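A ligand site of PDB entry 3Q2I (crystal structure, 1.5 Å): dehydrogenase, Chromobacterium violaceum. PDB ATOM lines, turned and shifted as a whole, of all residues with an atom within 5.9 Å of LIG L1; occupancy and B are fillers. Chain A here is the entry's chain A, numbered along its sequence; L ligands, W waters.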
ATOM      1  N   ARG A  23     -18.272 -33.059  -2.438  1.00  0.00           N
ATOM      2  CA  ARG A  23     -19.660 -33.140  -2.819  1.00  0.00           C
ATOM      3  C   ARG A  23     -19.904 -33.267  -4.313  1.00  0.00           C
ATOM      4  O   ARG A  23     -20.587 -34.231  -4.740  1.00  0.00           O
ATOM      5  CB  ARG A  23     -20.452 -31.995  -2.152  1.00  0.00           C
ATOM      6  CG  ARG A  23     -21.973 -32.125  -2.168  1.00  0.00           C
ATOM      7  CD  ARG A  23     -22.633 -30.937  -1.442  1.00  0.00           C
ATOM      8  NE  ARG A  23     -22.037 -30.746  -0.123  1.00  0.00           N
ATOM      9  CZ  ARG A  23     -22.068 -29.629   0.605  1.00  0.00           C
ATOM     10  NH1 ARG A  23     -22.657 -28.504   0.152  1.00  0.00           N
ATOM     11  NH2 ARG A  23     -21.507 -29.641   1.804  1.00  0.00           N
ATOM     12  N   LYS A 106     -17.204 -24.787 -11.968  1.00  0.00           N
ATOM     13  CA  LYS A 106     -17.544 -23.358 -11.873  1.00  0.00           C
ATOM     14  C   LYS A 106     -17.444 -22.957 -10.411  1.00  0.00           C
ATOM     15  O   LYS A 106     -17.539 -23.769  -9.494  1.00  0.00           O
ATOM     16  CB  LYS A 106     -18.955 -23.124 -12.399  1.00  0.00           C
ATOM     17  CG  LYS A 106     -20.045 -23.817 -11.564  1.00  0.00           C
ATOM     18  CD  LYS A 106     -20.314 -23.112 -10.225  1.00  0.00           C
ATOM     19  CE  LYS A 106     -21.762 -23.242  -9.780  1.00  0.00           C
ATOM     20  NZ  LYS A 106     -22.046 -22.614  -8.401  1.00  0.00           N
ATOM     21  N   GLN A 134     -23.157 -26.906 -16.719  1.00  0.00           N
ATOM     22  CA  GLN A 134     -23.976 -28.052 -17.094  1.00  0.00           C
ATOM     23  C   GLN A 134     -25.452 -27.705 -17.254  1.00  0.00           C
ATOM     24  O   GLN A 134     -26.226 -28.469 -17.848  1.00  0.00           O
ATOM     25  CB  GLN A 134     -23.681 -29.225 -16.154  1.00  0.00           C
ATOM     26  CG  GLN A 134     -24.475 -29.247 -14.852  1.00  0.00           C
ATOM     27  CD  GLN A 134     -23.972 -28.256 -13.842  1.00  0.00           C
ATOM     28  OE1 GLN A 134     -22.992 -27.554 -14.081  1.00  0.00           O
ATOM     29  NE2 GLN A 134     -24.611 -28.226 -12.684  1.00  0.00           N
ATOM     30  N   ASN A 135     -25.886 -26.548 -16.749  1.00  0.00           N
ATOM     31  CA  ASN A 135     -27.300 -26.156 -16.845  1.00  0.00           C
ATOM     32  C   ASN A 135     -27.782 -25.685 -18.213  1.00  0.00           C
ATOM     33  O   ASN A 135     -28.983 -25.639 -18.486  1.00  0.00           O
ATOM     34  CB  ASN A 135     -27.587 -25.039 -15.818  1.00  0.00           C
ATOM     35  CG  ASN A 135     -28.611 -25.411 -14.757  1.00  0.00           C
ATOM     36  OD1 ASN A 135     -28.742 -26.580 -14.367  1.00  0.00           O
ATOM     37  ND2 ASN A 135     -29.293 -24.389 -14.206  1.00  0.00           N
ATOM     38  N   TRP A 165     -33.681 -18.444  -2.956  1.00  0.00           N
ATOM     39  CA  TRP A 165     -33.334 -19.754  -2.456  1.00  0.00           C
ATOM     40  C   TRP A 165     -33.008 -19.714  -0.970  1.00  0.00           C
ATOM     41  O   TRP A 165     -33.072 -18.673  -0.303  1.00  0.00           O
ATOM     42  CB  TRP A 165     -32.116 -20.273  -3.248  1.00  0.00           C
ATOM     43  CG  TRP A 165     -32.441 -20.806  -4.635  1.00  0.00           C
ATOM     44  CD1 TRP A 165     -33.664 -20.909  -5.294  1.00  0.00           C
ATOM     45  CD2 TRP A 165     -31.471 -21.360  -5.519  1.00  0.00           C
ATOM     46  NE1 TRP A 165     -33.483 -21.468  -6.534  1.00  0.00           N
ATOM     47  CE2 TRP A 165     -32.140 -21.732  -6.708  1.00  0.00           C
ATOM     48  CE3 TRP A 165     -30.081 -21.506  -5.445  1.00  0.00           C
ATOM     49  CZ2 TRP A 165     -31.460 -22.297  -7.788  1.00  0.00           C
ATOM     50  CZ3 TRP A 165     -29.394 -22.077  -6.526  1.00  0.00           C
ATOM     51  CH2 TRP A 165     -30.091 -22.466  -7.696  1.00  0.00           C
ATOM     52  N   THR A 166     -32.612 -20.874  -0.430  1.00  0.00           N
ATOM     53  CA  THR A 166     -32.406 -20.935   0.997  1.00  0.00           C
ATOM     54  C   THR A 166     -31.154 -21.688   1.342  1.00  0.00           C
ATOM     55  O   THR A 166     -31.013 -22.831   0.908  1.00  0.00           O
ATOM     56  CB  THR A 166     -33.572 -21.710   1.672  1.00  0.00           C
ATOM     57  OG1 THR A 166     -34.809 -21.129   1.279  1.00  0.00           O
ATOM     58  CG2 THR A 166     -33.380 -21.689   3.173  1.00  0.00           C
ATOM     59  N   ARG A 167     -30.238 -21.076   2.107  1.00  0.00           N
ATOM     60  CA  ARG A 167     -29.005 -21.730   2.560  1.00  0.00           C
ATOM     61  C   ARG A 167     -28.857 -21.350   4.016  1.00  0.00           C
ATOM     62  O   ARG A 167     -28.747 -20.176   4.369  1.00  0.00           O
ATOM     63  CB  ARG A 167     -27.744 -21.243   1.825  1.00  0.00           C
ATOM     64  CG  ARG A 167     -27.742 -21.503   0.347  1.00  0.00           C
ATOM     65  CD  ARG A 167     -27.778 -22.994   0.044  1.00  0.00           C
ATOM     66  NE  ARG A 167     -27.660 -23.296  -1.376  1.00  0.00           N
ATOM     67  CZ  ARG A 167     -28.681 -23.440  -2.186  1.00  0.00           C
ATOM     68  NH1 ARG A 167     -28.454 -23.752  -3.463  1.00  0.00           N
ATOM     69  NH2 ARG A 167     -29.939 -23.272  -1.768  1.00  0.00           N
ATOM     70  N   PRO A 168     -28.922 -22.355   4.923  1.00  0.00           N
ATOM     71  CA  PRO A 168     -28.841 -22.046   6.342  1.00  0.00           C
ATOM     72  C   PRO A 168     -27.379 -21.916   6.757  1.00  0.00           C
ATOM     73  O   PRO A 168     -26.491 -22.272   5.959  1.00  0.00           O
ATOM     74  CB  PRO A 168     -29.462 -23.315   6.990  1.00  0.00           C
ATOM     75  CG  PRO A 168     -29.058 -24.414   6.009  1.00  0.00           C
ATOM     76  CD  PRO A 168     -29.245 -23.762   4.650  1.00  0.00           C
ATOM     77  N   GLU A 170     -25.580 -23.770   8.514  1.00  0.00           N
ATOM     78  CA  GLU A 170     -24.852 -25.037   8.541  1.00  0.00           C
ATOM     79  C   GLU A 170     -24.279 -25.373   7.148  1.00  0.00           C
ATOM     80  O   GLU A 170     -23.232 -26.015   7.037  1.00  0.00           O
ATOM     81  CB  GLU A 170     -25.741 -26.196   9.040  1.00  0.00           C
ATOM     82  CG  GLU A 170     -26.979 -26.444   8.209  1.00  0.00           C
ATOM     83  CD  GLU A 170     -27.564 -27.842   8.369  1.00  0.00           C
ATOM     84  OE1 GLU A 170     -28.529 -28.169   7.620  1.00  0.00           O
ATOM     85  OE2 GLU A 170     -27.086 -28.603   9.238  1.00  0.00           O
ATOM     86  N   TYR A 171     -24.903 -24.849   6.080  1.00  0.00           N
ATOM     87  CA  TYR A 171     -24.358 -24.997   4.727  1.00  0.00           C
ATOM     88  C   TYR A 171     -22.967 -24.363   4.615  1.00  0.00           C
ATOM     89  O   TYR A 171     -22.018 -24.954   4.082  1.00  0.00           O
ATOM     90  CB  TYR A 171     -25.358 -24.370   3.729  1.00  0.00           C
ATOM     91  CG  TYR A 171     -24.767 -24.097   2.376  1.00  0.00           C
ATOM     92  CD1 TYR A 171     -24.708 -25.076   1.394  1.00  0.00           C
ATOM     93  CD2 TYR A 171     -24.167 -22.866   2.088  1.00  0.00           C
ATOM     94  CE1 TYR A 171     -24.132 -24.855   0.155  1.00  0.00           C
ATOM     95  CE2 TYR A 171     -23.568 -22.642   0.869  1.00  0.00           C
ATOM     96  CZ  TYR A 171     -23.564 -23.607  -0.098  1.00  0.00           C
ATOM     97  OH  TYR A 171     -22.985 -23.363  -1.303  1.00  0.00           O
ATOM     98  N   ARG A 178     -15.911 -22.161   2.522  1.00  0.00           N
ATOM     99  CA  ARG A 178     -17.214 -21.710   2.053  1.00  0.00           C
ATOM    100  C   ARG A 178     -17.504 -20.354   2.721  1.00  0.00           C
ATOM    101  O   ARG A 178     -17.174 -20.145   3.886  1.00  0.00           O
ATOM    102  CB  ARG A 178     -18.310 -22.699   2.468  1.00  0.00           C
ATOM    103  CG  ARG A 178     -18.229 -24.023   1.636  1.00  0.00           C
ATOM    104  CD  ARG A 178     -19.330 -24.942   2.163  1.00  0.00           C
ATOM    105  NE  ARG A 178     -19.250 -26.267   1.523  1.00  0.00           N
ATOM    106  CZ  ARG A 178     -19.580 -26.527   0.269  1.00  0.00           C
ATOM    107  NH1 ARG A 178     -19.486 -27.792  -0.191  1.00  0.00           N
ATOM    108  NH2 ARG A 178     -19.952 -25.559  -0.576  1.00  0.00           N
ATOM    109  N   ASN A 190     -21.285 -17.970  -6.280  1.00  0.00           N
ATOM    110  CA  ASN A 190     -21.524 -19.409  -6.026  1.00  0.00           C
ATOM    111  C   ASN A 190     -22.961 -19.761  -6.395  1.00  0.00           C
ATOM    112  O   ASN A 190     -23.216 -20.232  -7.504  1.00  0.00           O
ATOM    113  CB  ASN A 190     -21.219 -19.799  -4.574  1.00  0.00           C
ATOM    114  CG  ASN A 190     -21.524 -21.284  -4.333  1.00  0.00           C
ATOM    115  OD1 ASN A 190     -22.370 -21.831  -5.021  1.00  0.00           O
ATOM    116  ND2 ASN A 190     -20.762 -21.951  -3.488  1.00  0.00           N
ATOM    117  N   GLN A 191     -23.924 -19.433  -5.536  1.00  0.00           N
ATOM    118  CA  GLN A 191     -25.216 -20.140  -5.623  1.00  0.00           C
ATOM    119  C   GLN A 191     -25.990 -19.894  -6.905  1.00  0.00           C
ATOM    120  O   GLN A 191     -26.482 -20.822  -7.572  1.00  0.00           O
ATOM    121  CB  GLN A 191     -26.071 -19.917  -4.371  1.00  0.00           C
ATOM    122  CG  GLN A 191     -25.474 -20.573  -3.129  1.00  0.00           C
ATOM    123  CD  GLN A 191     -24.429 -19.694  -2.454  1.00  0.00           C
ATOM    124  OE1 GLN A 191     -24.466 -18.460  -2.519  1.00  0.00           O
ATOM    125  NE2 GLN A 191     -23.480 -20.325  -1.797  1.00  0.00           N
ATOM    126  N   ALA A 192     -26.041 -18.631  -7.310  1.00  0.00           N
ATOM    127  CA  ALA A 192     -26.785 -18.277  -8.507  1.00  0.00           C
ATOM    128  C   ALA A 192     -25.945 -18.159  -9.788  1.00  0.00           C
ATOM    129  O   ALA A 192     -26.390 -17.541 -10.761  1.00  0.00           O
ATOM    130  CB  ALA A 192     -27.548 -16.955  -8.220  1.00  0.00           C
ATOM    131  N   SER A 193     -24.719 -18.692  -9.813  1.00  0.00           N
ATOM    132  CA  SER A 193     -23.845 -18.463 -10.937  1.00  0.00           C
ATOM    133  C   SER A 193     -24.400 -18.990 -12.268  1.00  0.00           C
ATOM    134  O   SER A 193     -24.085 -18.419 -13.296  1.00  0.00           O
ATOM    135  CB  SER A 193     -22.410 -18.964 -10.696  1.00  0.00           C
ATOM    136  OG  SER A 193     -22.510 -20.333 -10.410  1.00  0.00           O
ATOM    137  N   HIS A 194     -25.204 -20.039 -12.235  1.00  0.00           N
ATOM    138  CA  HIS A 194     -25.788 -20.572 -13.474  1.00  0.00           C
ATOM    139  C   HIS A 194     -26.858 -19.642 -14.037  1.00  0.00           C
ATOM    140  O   HIS A 194     -27.306 -19.816 -15.171  1.00  0.00           O
ATOM    141  CB  HIS A 194     -26.357 -21.990 -13.277  1.00  0.00           C
ATOM    142  CG  HIS A 194     -25.341 -23.047 -12.952  1.00  0.00           C
ATOM    143  ND1 HIS A 194     -24.382 -23.456 -13.844  1.00  0.00           N
ATOM    144  CD2 HIS A 194     -25.221 -23.881 -11.890  1.00  0.00           C
ATOM    145  CE1 HIS A 194     -23.649 -24.418 -13.315  1.00  0.00           C
ATOM    146  NE2 HIS A 194     -24.137 -24.700 -12.121  1.00  0.00           N
ATOM    147  N   TYR A 195     -27.340 -18.711 -13.209  1.00  0.00           N
ATOM    148  CA  TYR A 195     -28.308 -17.711 -13.646  1.00  0.00           C
ATOM    149  C   TYR A 195     -27.590 -16.445 -14.108  1.00  0.00           C
ATOM    150  O   TYR A 195     -28.009 -15.840 -15.096  1.00  0.00           O
ATOM    151  CB  TYR A 195     -29.310 -17.406 -12.525  1.00  0.00           C
ATOM    152  CG  TYR A 195     -30.174 -18.597 -12.154  1.00  0.00           C
ATOM    153  CD1 TYR A 195     -31.507 -18.692 -12.551  1.00  0.00           C
ATOM    154  CD2 TYR A 195     -29.651 -19.619 -11.368  1.00  0.00           C
ATOM    155  CE1 TYR A 195     -32.265 -19.801 -12.225  1.00  0.00           C
ATOM    156  CE2 TYR A 195     -30.417 -20.749 -11.044  1.00  0.00           C
ATOM    157  CZ  TYR A 195     -31.717 -20.816 -11.490  1.00  0.00           C
ATOM    158  OH  TYR A 195     -32.471 -21.969 -11.202  1.00  0.00           O
ATOM    159  N   PRO A 248     -39.406 -20.592   3.713  1.00  0.00           N
ATOM    160  CA  PRO A 248     -38.517 -21.352   4.576  1.00  0.00           C
ATOM    161  C   PRO A 248     -37.673 -22.336   3.778  1.00  0.00           C
ATOM    162  O   PRO A 248     -36.866 -23.060   4.369  1.00  0.00           O
ATOM    163  CB  PRO A 248     -39.512 -22.191   5.404  1.00  0.00           C
ATOM    164  CG  PRO A 248     -40.536 -22.507   4.396  1.00  0.00           C
ATOM    165  CD  PRO A 248     -40.636 -21.349   3.412  1.00  0.00           C
ATOM    166  N   LYS A 249     -37.860 -22.349   2.460  1.00  0.00           N
ATOM    167  CA  LYS A 249     -37.062 -23.185   1.545  1.00  0.00           C
ATOM    168  C   LYS A 249     -37.018 -22.543   0.150  1.00  0.00           C
ATOM    169  O   LYS A 249     -37.636 -21.496  -0.059  1.00  0.00           O
ATOM    170  CB  LYS A 249     -37.685 -24.595   1.453  1.00  0.00           C
ATOM    171  CG  LYS A 249     -39.060 -24.609   0.817  1.00  0.00           C
ATOM    172  CD  LYS A 249     -39.666 -26.022   0.885  1.00  0.00           C
ATOM    173  CE  LYS A 249     -41.125 -25.926   0.534  1.00  0.00           C
ATOM    174  NZ  LYS A 249     -41.186 -25.898  -0.937  1.00  0.00           N
ATOM    175  N   ASN A 250     -36.316 -23.157  -0.797  1.00  0.00           N
ATOM    176  CA  ASN A 250     -36.192 -22.605  -2.140  1.00  0.00           C
ATOM    177  C   ASN A 250     -37.562 -22.278  -2.715  1.00  0.00           C
ATOM    178  O   ASN A 250     -38.489 -23.106  -2.701  1.00  0.00           O
ATOM    179  CB  ASN A 250     -35.465 -23.537  -3.116  1.00  0.00           C
ATOM    180  CG  ASN A 250     -33.958 -23.582  -2.923  1.00  0.00           C
ATOM    181  OD1 ASN A 250     -33.399 -23.043  -1.964  1.00  0.00           O
ATOM    182  ND2 ASN A 250     -33.279 -24.229  -3.883  1.00  0.00           N
HETATM  183  N1  LIG L   1     -30.841 -26.043   0.779  1.00  0.00           N
HETATM  184  C1  LIG L   1     -31.667 -25.666   1.758  1.00  0.00           C
HETATM  185  O1  LIG L   1     -31.232 -25.555   2.933  1.00  0.00           O
HETATM  186  N2  LIG L   1     -32.953 -25.413   1.511  1.00  0.00           N
HETATM  187  C2  LIG L   1     -33.448 -25.541   0.277  1.00  0.00           C
HETATM  188  O2  LIG L   1     -34.687 -25.361   0.128  1.00  0.00           O
HETATM  189  C3  LIG L   1     -32.613 -25.938  -0.767  1.00  0.00           C
HETATM  190  C4  LIG L   1     -31.282 -26.200  -0.474  1.00  0.00           C
HETATM  191  P1  LIG L   1     -29.097 -28.192  -3.564  1.00  0.00           P
HETATM  192  P2  LIG L   1     -27.564 -28.096  -5.925  1.00  0.00           P
HETATM  193  O3  LIG L   1     -25.537 -23.926  -3.123  1.00  0.00           O
HETATM  194  O4  LIG L   1     -23.628 -24.999  -3.333  1.00  0.00           O
HETATM  195  C5  LIG L   1     -27.184 -25.540  -6.415  1.00  0.00           C
HETATM  196  O5  LIG L   1     -30.474 -27.777  -4.065  1.00  0.00           O
HETATM  197  O6  LIG L   1     -28.862 -28.064  -6.701  1.00  0.00           O
HETATM  198  C6  LIG L   1     -29.420 -26.242   1.106  1.00  0.00           C
HETATM  199  C7  LIG L   1     -26.687 -24.779  -7.658  1.00  0.00           C
HETATM  200  N3  LIG L   1     -27.013 -25.502  -8.882  1.00  0.00           N
HETATM  201  O7  LIG L   1     -28.735 -29.628  -3.327  1.00  0.00           O
HETATM  202  O8  LIG L   1     -26.636 -29.297  -5.910  1.00  0.00           O
HETATM  203  C8  LIG L   1     -29.093 -27.658   1.561  1.00  0.00           C
HETATM  204  O9  LIG L   1     -28.140 -27.491   2.621  1.00  0.00           O
HETATM  205  C9  LIG L   1     -25.181 -24.564  -7.588  1.00  0.00           C
HETATM  206  O10 LIG L   1     -24.868 -23.567  -8.592  1.00  0.00           O
HETATM  207  O11 LIG L   1     -27.921 -27.558  -4.454  1.00  0.00           O
HETATM  208  O12 LIG L   1     -26.634 -26.873  -6.478  1.00  0.00           O
HETATM  209  C10 LIG L   1     -28.357 -28.245   0.374  1.00  0.00           C
HETATM  210  O13 LIG L   1     -27.390 -29.212   0.786  1.00  0.00           O
HETATM  211  C11 LIG L   1     -24.751 -24.010  -6.214  1.00  0.00           C
HETATM  212  O14 LIG L   1     -23.343 -23.960  -6.061  1.00  0.00           O
HETATM  213  C12 LIG L   1     -27.660 -27.044  -0.269  1.00  0.00           C
HETATM  214  O15 LIG L   1     -28.681 -26.052  -0.107  1.00  0.00           O
HETATM  215  C13 LIG L   1     -25.232 -25.036  -5.163  1.00  0.00           C
HETATM  216  O16 LIG L   1     -26.658 -24.971  -5.217  1.00  0.00           O
HETATM  217  C14 LIG L   1     -27.473 -27.280  -1.755  1.00  0.00           C
HETATM  218  O17 LIG L   1     -28.811 -27.364  -2.221  1.00  0.00           O
HETATM  219  C15 LIG L   1     -24.755 -24.649  -3.787  1.00  0.00           C
HETATM  220  C16 LIG L   1     -27.764 -25.068  -9.894  1.00  0.00           C
HETATM  221  O18 LIG L   1     -28.226 -23.930 -10.029  1.00  0.00           O
HETATM  222  C17 LIG L   1     -28.045 -26.085 -10.972  1.00  0.00           C
HETATM  223  P1  LG2 L   2     -16.385 -29.725  -1.009  1.00  0.00           P
HETATM  224  O1  LG2 L   2     -15.913 -28.933   0.144  1.00  0.00           O
HETATM  225  O2  LG2 L   2     -17.519 -30.816  -0.809  1.00  0.00           O
HETATM  226  O3  LG2 L   2     -15.213 -30.477  -1.763  1.00  0.00           O
HETATM  227  C1  LG2 L   2     -13.971 -30.105  -1.237  1.00  0.00           C
HETATM  228  C2  LG2 L   2     -12.943 -31.124  -1.698  1.00  0.00           C
HETATM  229  O4  LG2 L   2     -11.695 -30.545  -2.134  1.00  0.00           O
HETATM  230  C3  LG2 L   2     -12.716 -31.704  -0.300  1.00  0.00           C
HETATM  231  O5  LG2 L   2     -12.832 -33.134  -0.325  1.00  0.00           O
HETATM  232  C4  LG2 L   2     -11.380 -31.104   0.164  1.00  0.00           C
HETATM  233  O6  LG2 L   2     -10.659 -31.911   1.091  1.00  0.00           O
HETATM  234  C5  LG2 L   2     -10.683 -31.045  -1.218  1.00  0.00           C
HETATM  235  N1  LG2 L   2      -9.501 -30.211  -1.237  1.00  0.00           N
HETATM  236  C6  LG2 L   2      -9.376 -28.953  -0.681  1.00  0.00           C
HETATM  237  N2  LG2 L   2      -8.192 -28.494  -0.969  1.00  0.00           N
HETATM  238  C7  LG2 L   2      -7.518 -29.367  -1.801  1.00  0.00           C
HETATM  239  C8  LG2 L   2      -6.247 -29.415  -2.404  1.00  0.00           C
HETATM  240  N3  LG2 L   2      -5.334 -28.393  -2.276  1.00  0.00           N
HETATM  241  N4  LG2 L   2      -5.918 -30.500  -3.125  1.00  0.00           N
HETATM  242  C9  LG2 L   2      -6.773 -31.497  -3.242  1.00  0.00           C
HETATM  243  N5  LG2 L   2      -7.993 -31.527  -2.704  1.00  0.00           N
HETATM  244  C10 LG2 L   2      -8.371 -30.466  -1.954  1.00  0.00           C
HETATM  245  O7  LG2 L   2     -16.921 -28.706  -2.109  1.00  0.00           O
HETATM  246  P2  LG2 L   2     -17.858 -28.966  -3.316  1.00  0.00           P
HETATM  247  O8  LG2 L   2     -19.273 -28.578  -2.997  1.00  0.00           O
HETATM  248  O9  LG2 L   2     -17.675 -30.354  -3.982  1.00  0.00           O
HETATM  249  O10 LG2 L   2     -17.565 -27.767  -4.380  1.00  0.00           O
HETATM  250  C11 LG2 L   2     -16.440 -28.100  -5.148  1.00  0.00           C
HETATM  251  C12 LG2 L   2     -16.305 -27.189  -6.357  1.00  0.00           C
HETATM  252  O11 LG2 L   2     -17.425 -27.520  -7.188  1.00  0.00           O
HETATM  253  C13 LG2 L   2     -16.524 -25.672  -6.064  1.00  0.00           C
HETATM  254  O12 LG2 L   2     -15.726 -24.965  -7.021  1.00  0.00           O
HETATM  255  C14 LG2 L   2     -18.001 -25.443  -6.394  1.00  0.00           C
HETATM  256  O13 LG2 L   2     -18.247 -24.125  -6.879  1.00  0.00           O
HETATM  257  C15 LG2 L   2     -18.266 -26.441  -7.561  1.00  0.00           C
HETATM  258  N6  LG2 L   2     -19.650 -26.843  -7.657  1.00  0.00           N
HETATM  259  C16 LG2 L   2     -20.265 -26.777  -8.825  1.00  0.00           C
HETATM  260  C17 LG2 L   2     -21.622 -27.087  -8.969  1.00  0.00           C
HETATM  261  C18 LG2 L   2     -22.289 -27.039 -10.289  1.00  0.00           C
HETATM  262  O14 LG2 L   2     -23.481 -26.862 -10.481  1.00  0.00           O
HETATM  263  N7  LG2 L   2     -21.545 -27.198 -11.422  1.00  0.00           N
HETATM  264  C19 LG2 L   2     -22.345 -27.365  -7.791  1.00  0.00           C
HETATM  265  C20 LG2 L   2     -21.640 -27.529  -6.613  1.00  0.00           C
HETATM  266  C21 LG2 L   2     -20.297 -27.256  -6.554  1.00  0.00           C
HETATM  267  O   HOH W   1     -20.927 -24.897  -4.225  1.00  0.00           O
HETATM  268  O   HOH W   2     -34.914 -25.100   3.575  1.00  0.00           O
HETATM  269  O   HOH W   3     -23.409 -27.645  -2.762  1.00  0.00           O
HETATM  270  O   HOH W   4     -36.322 -27.271  -1.031  1.00  0.00           O
HETATM  271  O   HOH W   5     -30.831 -24.794  -4.606  1.00  0.00           O
HETATM  272  O   HOH W   6     -26.906 -21.401 -10.125  1.00  0.00           O
HETATM  273  O   HOH W   7     -31.157 -24.054 -10.675  1.00  0.00           O
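OD1 of Asn 190 is in hydrogen-bond range of O14 of LIG L1 (2.6 Å). A nitrogen (N2) of LIG L1 sits close to the backbone carbonyl oxygen (O) of Thr 166 (3.3 Å). The side-chain hydroxyl (OH) of Tyr 171 lies within hydrogen-bond range of an oxygen (O4) of LIG L1. The backbone carbonyl oxygen (O) of Lys 106 sits at hydrogen-bond distance from an oxygen (O13) of LG2 L2 (2.7 Å). An oxygen (O2) of LIG L1 sits at hydrogen-bond distance from the backbone NH (N) of Asn 250 (2.9 Å). N of Arg 23 sits at hydrogen-bond distance from O2 of LG2 L2, at 2.9 Å. The backbone carbonyl oxygen (O) of Gln 191 lies within hydrogen-bond range of an oxygen (O10) of LIG L1 (3.3 Å). NZ of Lys 106 lies within hydrogen-bond range of O10 of LIG L1 (3.0 Å). NH1 of Arg 178 is in salt-bridge range of O8 of LG2 L2, at 2.9 Å. A ring nitrogen (NE2) of His 194 sits at hydrogen-bond distance from an oxygen (O14) of LG2 L2 (2.8 Å). OD1 of Asn 250 lies close to O2 of LIG L1, 3.4 Å away. NE of Arg 167 is in salt-bridge range of O3 of LIG L1 (2.8 Å). An oxygen (O14) of LG2 L2 lies within hydrogen-bond range of the side-chain amide nitrogen of Gln 134, at 2.8 Å.
NZ of Lys 106 lies close to OG of Ser 193 (3.1 Å). NE2 of Gln 191 sits at hydrogen-bond distance from OH of Tyr 171. O of Asn 190 is in hydrogen-bond range of OG of Ser 193, 3.0 Å away. OH of Tyr 171 is in hydrogen-bond range of ND2 of Asn 190 (3.4 Å). OG1 of Thr 166 sits close to O of Lys 249, 3.1 Å away. NZ of Lys 106 lies within hydrogen-bond range of O of Asn 190 (2.8 Å). OD1 of Asn 250 lies within hydrogen-bond range of NH2 of Arg 167 (3.5 Å). The side-chain amide oxygen (OD1) of Asn 250 is in hydrogen-bond range of the backbone NH (N) of Thr 166 (2.8 Å).
Asn 135 touches LIG L1. Trp 165 touches LIG L1. CD of Pro 168 touches O1 of LIG L1, at 3.2 Å. CD2 of His 194 touches O10 of LIG L1, 3.3 Å away. Tyr 195 touches LIG L1. CB of Lys 249 touches O2 of LIG L1, 3.4 Å away. Of the 20 residues printed, 13 come within 4 Å of LIG L1. The nearest printed residue that does not touch LIG L1 is Gln 134 (4.4 Å).
Water W3 lies within hydrogen-bond range of an oxygen (O4) of LIG L1 (2.7 Å) and the guanidinium group of Arg 23 (3.1 Å). Water W1 bridges an oxygen (O4) of LIG L1 (2.8 Å) and the side-chain amide nitrogen (ND2) of Asn 190 (3.0 Å). Water W6 lies within hydrogen-bond range of O of Gln 191 (2.7 Å), O18 of LIG L1 (2.9 Å), N of His 194 (3.0 Å) and N of Ser 193 (3.5 Å). Water W2 bridges N2 of LIG L1 and O of Pro 248. Water W7 bridges the side-chain hydroxyl of Tyr 195 and an oxygen (O18) of LIG L1. Water W5 lies within hydrogen-bond range of ND2 of Asn 250, NH1 of Arg 167 and O5 of LIG L1.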
